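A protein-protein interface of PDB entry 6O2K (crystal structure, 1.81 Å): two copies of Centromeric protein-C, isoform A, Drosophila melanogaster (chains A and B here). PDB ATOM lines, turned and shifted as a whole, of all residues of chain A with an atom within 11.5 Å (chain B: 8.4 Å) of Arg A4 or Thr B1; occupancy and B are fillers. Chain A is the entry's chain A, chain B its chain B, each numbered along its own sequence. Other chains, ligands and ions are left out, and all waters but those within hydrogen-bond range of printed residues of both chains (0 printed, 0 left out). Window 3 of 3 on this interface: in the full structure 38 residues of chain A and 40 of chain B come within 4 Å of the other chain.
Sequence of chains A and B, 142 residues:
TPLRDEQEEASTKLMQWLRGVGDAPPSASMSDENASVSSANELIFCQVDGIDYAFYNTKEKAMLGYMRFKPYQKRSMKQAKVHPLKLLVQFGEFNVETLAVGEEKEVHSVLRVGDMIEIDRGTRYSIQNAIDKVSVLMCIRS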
ATOM      1  N   ARG A   4     -24.208  -4.296   5.568  1.00  0.00           N
ATOM      2  CA  ARG A   4     -24.426  -2.866   5.811  1.00  0.00           C
ATOM      3  C   ARG A   4     -25.487  -2.638   6.883  1.00  0.00           C
ATOM      4  O   ARG A   4     -26.439  -3.413   6.992  1.00  0.00           O
ATOM      5  CB  ARG A   4     -24.853  -2.147   4.529  1.00  0.00           C
ATOM      6  CG  ARG A   4     -23.859  -2.160   3.379  1.00  0.00           C
ATOM      7  CD  ARG A   4     -24.386  -1.242   2.278  1.00  0.00           C
ATOM      8  NE  ARG A   4     -23.483  -1.102   1.140  1.00  0.00           N
ATOM      9  CZ  ARG A   4     -23.728  -1.605  -0.066  1.00  0.00           C
ATOM     10  NH1 ARG A   4     -24.845  -2.288  -0.286  1.00  0.00           N
ATOM     11  NH2 ARG A   4     -22.854  -1.432  -1.049  1.00  0.00           N
ATOM     12  N   ASP A   5     -25.335  -1.567   7.663  1.00  0.00           N
ATOM     13  CA  ASP A   5     -26.352  -1.199   8.640  1.00  0.00           C
ATOM     14  C   ASP A   5     -27.435  -0.370   7.946  1.00  0.00           C
ATOM     15  O   ASP A   5     -27.439  -0.205   6.721  1.00  0.00           O
ATOM     16  CB  ASP A   5     -25.714  -0.490   9.837  1.00  0.00           C
ATOM     17  CG  ASP A   5     -25.021   0.823   9.470  1.00  0.00           C
ATOM     18  OD1 ASP A   5     -25.490   1.551   8.567  1.00  0.00           O
ATOM     19  OD2 ASP A   5     -23.991   1.135  10.109  1.00  0.00           O
ATOM     20  N   GLU A   6     -28.367   0.175   8.728  1.00  0.00           N
ATOM     21  CA  GLU A   6     -29.508   0.868   8.136  1.00  0.00           C
ATOM     22  C   GLU A   6     -29.084   2.144   7.410  1.00  0.00           C
ATOM     23  O   GLU A   6     -29.622   2.462   6.340  1.00  0.00           O
ATOM     24  CB  GLU A   6     -30.545   1.165   9.219  1.00  0.00           C
ATOM     25  CG  GLU A   6     -31.813   1.814   8.703  1.00  0.00           C
ATOM     26  CD  GLU A   6     -32.691   2.344   9.823  1.00  0.00           C
ATOM     27  OE1 GLU A   6     -33.883   2.620   9.567  1.00  0.00           O
ATOM     28  OE2 GLU A   6     -32.193   2.474  10.961  1.00  0.00           O
ATOM     29  N   GLN A   7     -28.105   2.877   7.955  1.00  0.00           N
ATOM     30  CA  GLN A   7     -27.714   4.153   7.354  1.00  0.00           C
ATOM     31  C   GLN A   7     -26.839   3.953   6.124  1.00  0.00           C
ATOM     32  O   GLN A   7     -26.964   4.698   5.144  1.00  0.00           O
ATOM     33  CB  GLN A   7     -26.983   5.027   8.370  1.00  0.00           C
ATOM     34  CG  GLN A   7     -27.909   5.769   9.317  1.00  0.00           C
ATOM     35  CD  GLN A   7     -28.441   4.856  10.394  1.00  0.00           C
ATOM     36  OE1 GLN A   7     -27.801   3.869  10.748  1.00  0.00           O
ATOM     37  NE2 GLN A   7     -29.618   5.171  10.912  1.00  0.00           N
ATOM     38  N   GLU A   8     -25.936   2.968   6.165  1.00  0.00           N
ATOM     39  CA  GLU A   8     -25.192   2.603   4.963  1.00  0.00           C
ATOM     40  C   GLU A   8     -26.144   2.146   3.862  1.00  0.00           C
ATOM     41  O   GLU A   8     -25.971   2.502   2.688  1.00  0.00           O
ATOM     42  CB  GLU A   8     -24.165   1.519   5.303  1.00  0.00           C
ATOM     43  CG  GLU A   8     -23.058   2.023   6.237  1.00  0.00           C
ATOM     44  CD  GLU A   8     -22.205   0.915   6.838  1.00  0.00           C
ATOM     45  OE1 GLU A   8     -22.770  -0.107   7.295  1.00  0.00           O
ATOM     46  OE2 GLU A   8     -20.962   1.073   6.860  1.00  0.00           O
ATOM     47  N   GLU A   9     -27.185   1.391   4.235  1.00  0.00           N
ATOM     48  CA  GLU A   9     -28.219   0.987   3.285  1.00  0.00           C
ATOM     49  C   GLU A   9     -28.906   2.194   2.667  1.00  0.00           C
ATOM     50  O   GLU A   9     -29.118   2.246   1.450  1.00  0.00           O
ATOM     51  CB  GLU A   9     -29.260   0.103   3.976  1.00  0.00           C
ATOM     52  CG  GLU A   9     -28.848  -1.348   4.176  1.00  0.00           C
ATOM     53  CD  GLU A   9     -28.436  -2.035   2.884  1.00  0.00           C
ATOM     54  OE1 GLU A   9     -27.578  -2.942   2.946  1.00  0.00           O
ATOM     55  OE2 GLU A   9     -28.971  -1.679   1.810  1.00  0.00           O
ATOM     56  N   ALA A  10     -29.300   3.160   3.506  1.00  0.00           N
ATOM     57  CA  ALA A  10     -29.984   4.347   3.003  1.00  0.00           C
ATOM     58  C   ALA A  10     -29.089   5.141   2.063  1.00  0.00           C
ATOM     59  O   ALA A  10     -29.543   5.641   1.021  1.00  0.00           O
ATOM     60  CB  ALA A  10     -30.450   5.211   4.174  1.00  0.00           C
ATOM     61  N   SER A  11     -27.810   5.265   2.406  1.00  0.00           N
ATOM     62  CA  SER A  11     -26.912   6.025   1.548  1.00  0.00           C
ATOM     63  C   SER A  11     -26.717   5.313   0.213  1.00  0.00           C
ATOM     64  O   SER A  11     -26.656   5.959  -0.845  1.00  0.00           O
ATOM     65  CB  SER A  11     -25.582   6.257   2.268  1.00  0.00           C
ATOM     66  OG  SER A  11     -24.522   6.408   1.349  1.00  0.00           O
ATOM     67  N   THR A  12     -26.669   3.977   0.236  1.00  0.00           N
ATOM     68  CA  THR A  12     -26.560   3.229  -1.015  1.00  0.00           C
ATOM     69  C   THR A  12     -27.808   3.390  -1.875  1.00  0.00           C
ATOM     70  O   THR A  12     -27.704   3.579  -3.096  1.00  0.00           O
ATOM     71  CB  THR A  12     -26.296   1.754  -0.724  1.00  0.00           C
ATOM     72  OG1 THR A  12     -25.036   1.628  -0.053  1.00  0.00           O
ATOM     73  CG2 THR A  12     -26.266   0.963  -2.020  1.00  0.00           C
ATOM     74  N   LYS A  13     -28.996   3.315  -1.262  1.00  0.00           N
ATOM     75  CA  LYS A  13     -30.226   3.527  -2.026  1.00  0.00           C
ATOM     76  C   LYS A  13     -30.249   4.909  -2.668  1.00  0.00           C
ATOM     77  O   LYS A  13     -30.633   5.058  -3.840  1.00  0.00           O
ATOM     78  CB  LYS A  13     -31.458   3.345  -1.139  1.00  0.00           C
ATOM     79  CG  LYS A  13     -32.774   3.673  -1.859  1.00  0.00           C
ATOM     80  CD  LYS A  13     -33.933   2.827  -1.345  1.00  0.00           C
ATOM     81  CE  LYS A  13     -35.000   2.620  -2.418  1.00  0.00           C
ATOM     82  NZ  LYS A  13     -34.849   1.314  -3.134  1.00  0.00           N
ATOM     83  N   LEU A  14     -29.840   5.935  -1.917  1.00  0.00           N
ATOM     84  CA  LEU A  14     -29.825   7.279  -2.480  1.00  0.00           C
ATOM     85  C   LEU A  14     -28.892   7.346  -3.678  1.00  0.00           C
ATOM     86  O   LEU A  14     -29.252   7.879  -4.738  1.00  0.00           O
ATOM     87  CB  LEU A  14     -29.406   8.295  -1.420  1.00  0.00           C
ATOM     88  CG  LEU A  14     -29.042   9.668  -1.990  1.00  0.00           C
ATOM     89  CD1 LEU A  14     -30.292  10.348  -2.534  1.00  0.00           C
ATOM     90  CD2 LEU A  14     -28.370  10.521  -0.950  1.00  0.00           C
ATOM     91  N   MET A  15     -27.683   6.792  -3.532  1.00  0.00           N
ATOM     92  CA  MET A  15     -26.710   6.885  -4.615  1.00  0.00           C
ATOM     93  C   MET A  15     -27.186   6.126  -5.846  1.00  0.00           C
ATOM     94  O   MET A  15     -27.013   6.597  -6.978  1.00  0.00           O
ATOM     95  CB  MET A  15     -25.351   6.357  -4.150  1.00  0.00           C
ATOM     96  CG  MET A  15     -24.196   6.769  -5.043  1.00  0.00           C
ATOM     97  SD  MET A  15     -24.133   8.535  -5.383  1.00  0.00           S
ATOM     98  CE  MET A  15     -23.880   9.174  -3.732  1.00  0.00           C
ATOM     99  N   GLN A  16     -27.797   4.958  -5.648  1.00  0.00           N
ATOM    100  CA  GLN A  16     -28.284   4.188  -6.789  1.00  0.00           C
ATOM    101  C   GLN A  16     -29.439   4.896  -7.489  1.00  0.00           C
ATOM    102  O   GLN A  16     -29.595   4.762  -8.709  1.00  0.00           O
ATOM    103  CB  GLN A  16     -28.698   2.795  -6.334  1.00  0.00           C
ATOM    104  CG  GLN A  16     -27.537   1.971  -5.859  1.00  0.00           C
ATOM    105  CD  GLN A  16     -27.943   0.564  -5.541  1.00  0.00           C
ATOM    106  OE1 GLN A  16     -29.001   0.332  -4.952  1.00  0.00           O
ATOM    107  NE2 GLN A  16     -27.106  -0.395  -5.926  1.00  0.00           N
ATOM    108  N   ARG A  19     -27.830   7.595  -9.555  1.00  0.00           N
ATOM    109  CA  ARG A  19     -27.140   7.007 -10.692  1.00  0.00           C
ATOM    110  C   ARG A  19     -28.104   6.460 -11.739  1.00  0.00           C
ATOM    111  O   ARG A  19     -27.669   6.100 -12.842  1.00  0.00           O
ATOM    112  CB  ARG A  19     -26.192   5.905 -10.200  1.00  0.00           C
ATOM    113  CG  ARG A  19     -24.968   6.449  -9.464  1.00  0.00           C
ATOM    114  CD  ARG A  19     -24.185   5.347  -8.738  1.00  0.00           C
ATOM    115  NE  ARG A  19     -23.718   4.291  -9.642  1.00  0.00           N
ATOM    116  CZ  ARG A  19     -23.211   3.126  -9.237  1.00  0.00           C
ATOM    117  NH1 ARG A  19     -23.099   2.862  -7.936  1.00  0.00           N
ATOM    118  NH2 ARG A  19     -22.812   2.222 -10.126  1.00  0.00           N
ATOM    119  N   VAL A  21     -29.997   3.680 -11.307  1.00  0.00           N
ATOM    120  CA  VAL A  21     -30.045   2.224 -11.241  1.00  0.00           C
ATOM    121  C   VAL A  21     -30.913   1.718 -10.103  1.00  0.00           C
ATOM    122  O   VAL A  21     -31.021   0.497  -9.919  1.00  0.00           O
ATOM    123  CB  VAL A  21     -28.629   1.622 -11.145  1.00  0.00           C
ATOM    124  CG1 VAL A  21     -27.765   2.137 -12.283  1.00  0.00           C
ATOM    125  CG2 VAL A  21     -27.992   1.956  -9.809  1.00  0.00           C
ATOM    126  N   PHE A  91     -20.549  11.310  -7.765  1.00  0.00           N
ATOM    127  CA  PHE A  91     -20.101   9.946  -8.047  1.00  0.00           C
ATOM    128  C   PHE A  91     -19.367   9.926  -9.379  1.00  0.00           C
ATOM    129  O   PHE A  91     -19.800  10.575 -10.331  1.00  0.00           O
ATOM    130  CB  PHE A  91     -21.293   8.974  -8.096  1.00  0.00           C
ATOM    131  CG  PHE A  91     -20.907   7.537  -8.289  1.00  0.00           C
ATOM    132  CD1 PHE A  91     -20.686   6.712  -7.202  1.00  0.00           C
ATOM    133  CD2 PHE A  91     -20.768   7.010  -9.557  1.00  0.00           C
ATOM    134  CE1 PHE A  91     -20.335   5.398  -7.369  1.00  0.00           C
ATOM    135  CE2 PHE A  91     -20.407   5.695  -9.732  1.00  0.00           C
ATOM    136  CZ  PHE A  91     -20.194   4.880  -8.635  1.00  0.00           C
ATOM    137  N   THR B   1     -23.443  -6.928   0.609  1.00  0.00           N
ATOM    138  CA  THR B   1     -22.584  -5.886   0.050  1.00  0.00           C
ATOM    139  C   THR B   1     -21.956  -6.360  -1.260  1.00  0.00           C
ATOM    140  O   THR B   1     -20.995  -7.132  -1.250  1.00  0.00           O
ATOM    141  CB  THR B   1     -21.469  -5.471   1.042  1.00  0.00           C
ATOM    142  OG1 THR B   1     -22.056  -4.898   2.218  1.00  0.00           O
ATOM    143  CG2 THR B   1     -20.530  -4.449   0.410  1.00  0.00           C
ATOM    144  N   PRO B   2     -22.512  -5.913  -2.386  1.00  0.00           N
ATOM    145  CA  PRO B   2     -21.950  -6.304  -3.686  1.00  0.00           C
ATOM    146  C   PRO B   2     -20.526  -5.793  -3.846  1.00  0.00           C
ATOM    147  O   PRO B   2     -20.222  -4.645  -3.513  1.00  0.00           O
ATOM    148  CB  PRO B   2     -22.903  -5.651  -4.696  1.00  0.00           C
ATOM    149  CG  PRO B   2     -23.568  -4.542  -3.933  1.00  0.00           C
ATOM    150  CD  PRO B   2     -23.691  -5.043  -2.527  1.00  0.00           C
ATOM    151  N   LEU B   3     -19.653  -6.667  -4.351  1.00  0.00           N
ATOM    152  CA  LEU B   3     -18.253  -6.328  -4.579  1.00  0.00           C
ATOM    153  C   LEU B   3     -18.132  -5.035  -5.367  1.00  0.00           C
ATOM    154  O   LEU B   3     -18.659  -4.918  -6.476  1.00  0.00           O
ATOM    155  CB  LEU B   3     -17.551  -7.471  -5.318  1.00  0.00           C
ATOM    156  CG  LEU B   3     -16.038  -7.327  -5.542  1.00  0.00           C
ATOM    157  CD1 LEU B   3     -15.280  -7.243  -4.226  1.00  0.00           C
ATOM    158  CD2 LEU B   3     -15.505  -8.479  -6.371  1.00  0.00           C
ATOM    159  N   ARG B   4     -17.429  -4.068  -4.783  1.00  0.00           N
ATOM    160  CA  ARG B   4     -17.379  -2.721  -5.327  1.00  0.00           C
ATOM    161  C   ARG B   4     -16.515  -2.636  -6.577  1.00  0.00           C
ATOM    162  O   ARG B   4     -15.481  -3.304  -6.688  1.00  0.00           O
ATOM    163  CB  ARG B   4     -16.827  -1.751  -4.284  1.00  0.00           C
ATOM    164  CG  ARG B   4     -17.774  -1.400  -3.156  1.00  0.00           C
ATOM    165  CD  ARG B   4     -17.054  -0.522  -2.153  1.00  0.00           C
ATOM    166  NE  ARG B   4     -17.838  -0.299  -0.943  1.00  0.00           N
ATOM    167  CZ  ARG B   4     -17.927  -1.166   0.058  1.00  0.00           C
ATOM    168  NH1 ARG B   4     -17.283  -2.325  -0.006  1.00  0.00           N
ATOM    169  NH2 ARG B   4     -18.663  -0.875   1.122  1.00  0.00           N
ATOM    170  N   GLU B   8     -17.038   2.893  -6.882  1.00  0.00           N
ATOM    171  CA  GLU B   8     -17.651   2.624  -5.588  1.00  0.00           C
ATOM    172  C   GLU B   8     -16.600   2.569  -4.484  1.00  0.00           C
ATOM    173  O   GLU B   8     -16.836   3.054  -3.374  1.00  0.00           O
ATOM    174  CB  GLU B   8     -18.454   1.325  -5.664  1.00  0.00           C
ATOM    175  CG  GLU B   8     -19.719   1.491  -6.504  1.00  0.00           C
ATOM    176  CD  GLU B   8     -20.466   0.195  -6.723  1.00  0.00           C
ATOM    177  OE1 GLU B   8     -19.816  -0.864  -6.850  1.00  0.00           O
ATOM    178  OE2 GLU B   8     -21.714   0.233  -6.760  1.00  0.00           O
ATOM    179  N   THR B  12     -16.675   5.074  -1.313  1.00  0.00           N
ATOM    180  CA  THR B  12     -16.658   4.542   0.042  1.00  0.00           C
ATOM    181  C   THR B  12     -15.461   5.065   0.831  1.00  0.00           C
ATOM    182  O   THR B  12     -15.583   5.365   2.024  1.00  0.00           O
ATOM    183  CB  THR B  12     -16.669   3.012  -0.019  1.00  0.00           C
ATOM    184  OG1 THR B  12     -18.002   2.577  -0.317  1.00  0.00           O
ATOM    185  CG2 THR B  12     -16.212   2.405   1.303  1.00  0.00           C
ATOM    186  N   PHE B  91     -24.452  11.662   5.486  1.00  0.00           N
ATOM    187  CA  PHE B  91     -24.535  10.329   6.070  1.00  0.00           C
ATOM    188  C   PHE B  91     -25.249  10.451   7.404  1.00  0.00           C
ATOM    189  O   PHE B  91     -25.007  11.398   8.154  1.00  0.00           O
ATOM    190  CB  PHE B  91     -23.144   9.700   6.271  1.00  0.00           C
ATOM    191  CG  PHE B  91     -23.185   8.270   6.750  1.00  0.00           C
ATOM    192  CD1 PHE B  91     -23.187   7.979   8.106  1.00  0.00           C
ATOM    193  CD2 PHE B  91     -23.240   7.219   5.846  1.00  0.00           C
ATOM    194  CE1 PHE B  91     -23.242   6.670   8.549  1.00  0.00           C
ATOM    195  CE2 PHE B  91     -23.281   5.897   6.282  1.00  0.00           C
ATOM    196  CZ  PHE B  91     -23.285   5.618   7.628  1.00  0.00           C
ATOM    197  N   LYS B 133     -24.404   6.751  15.854  1.00  0.00           N
ATOM    198  CA  LYS B 133     -23.240   6.655  14.986  1.00  0.00           C
ATOM    199  C   LYS B 133     -22.845   8.059  14.552  1.00  0.00           C
ATOM    200  O   LYS B 133     -23.633   9.005  14.643  1.00  0.00           O
ATOM    201  CB  LYS B 133     -23.518   5.802  13.745  1.00  0.00           C
ATOM    202  CG  LYS B 133     -24.067   4.416  14.013  1.00  0.00           C
ATOM    203  CD  LYS B 133     -24.731   3.839  12.763  1.00  0.00           C
ATOM    204  CE  LYS B 133     -24.096   4.386  11.491  1.00  0.00           C
ATOM    205  NZ  LYS B 133     -22.978   3.529  11.013  1.00  0.00           N
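Arg A4 touches just these residues of chain B: Thr B1 (3.5 Å) and Pro B2 (3.7 Å).
Of the printed residues of chain B, Asp A5 touches Lys B133 (2.8 Å).
Printed residues of chain B within 4 Å of Gln A7: Phe B91 (3.8 Å) and Lys B133 (3.7 Å).
Of the printed residues of chain B, Glu A8 touches Phe B91.
Lys A13 touches none of the printed residues of chain B.
Of the printed residues of chain B, Arg A19 touches Glu B8 (3.2 Å).
Phe A91 touches none of the printed residues of chain B.
Of chain A, only Arg A4 comes within 4 Å of Thr B1.
Of the printed residues of chain A, Glu B8 touches Arg A19.
The nearest residue of chain B that does not touch Arg A4 is Arg B4 (4.8 Å).
The nearest printed residue of chain A that does not touch Lys B133 is Glu A8 (5.0 Å).
Among the printed residues, merely in contact across the chains: Arg A4 with Thr B1 (3.5 Å), Arg A4 with Pro B2 (3.7 Å), Gln A7 with Phe B91 (3.8 Å), Gln A7 with Lys B133 (3.7 Å) and Glu A8 with Phe B91 (3.9 Å).
Glu A8 touches Phe B91, but with the chains exchanged Phe A91 does not touch Glu B8 (4.03 Å).
OG1 of Thr A12 sits at hydrogen-bond distance from NE of Arg A4 (3.4 Å).
OD1 of Asp A5 is in hydrogen-bond range of N of Gln A7, 3.0 Å away.
The side-chain carboxylate of Asp A5 is in hydrogen-bond range of the backbone NH of Glu A8, at 2.8 Å.
O of Glu A8 sits at hydrogen-bond distance from OG1 of Thr A12, at 3.0 Å.
O of Glu B8 lies within hydrogen-bond range of OG1 of Thr B12 (3.3 Å).
The side-chain carboxylate of Asp A5 lies within salt-bridge range of the side-chain amino group of Lys B133 (2.8 Å).
The guanidinium group of Arg A19 is in salt-bridge range of the side-chain carboxylate of Glu B8 (3.2 Å).
Hydrophobic or aromatic side chains of chain B within 4 Å of the printed part of chain A: Pro B2 and Phe B91.
Among the printed residues, Asp or Glu carboxylates within 4 Å of a Lys or Arg side-chain nitrogen of the other chain: Asp A5 with Lys B133 and Arg A19 with Glu B8.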
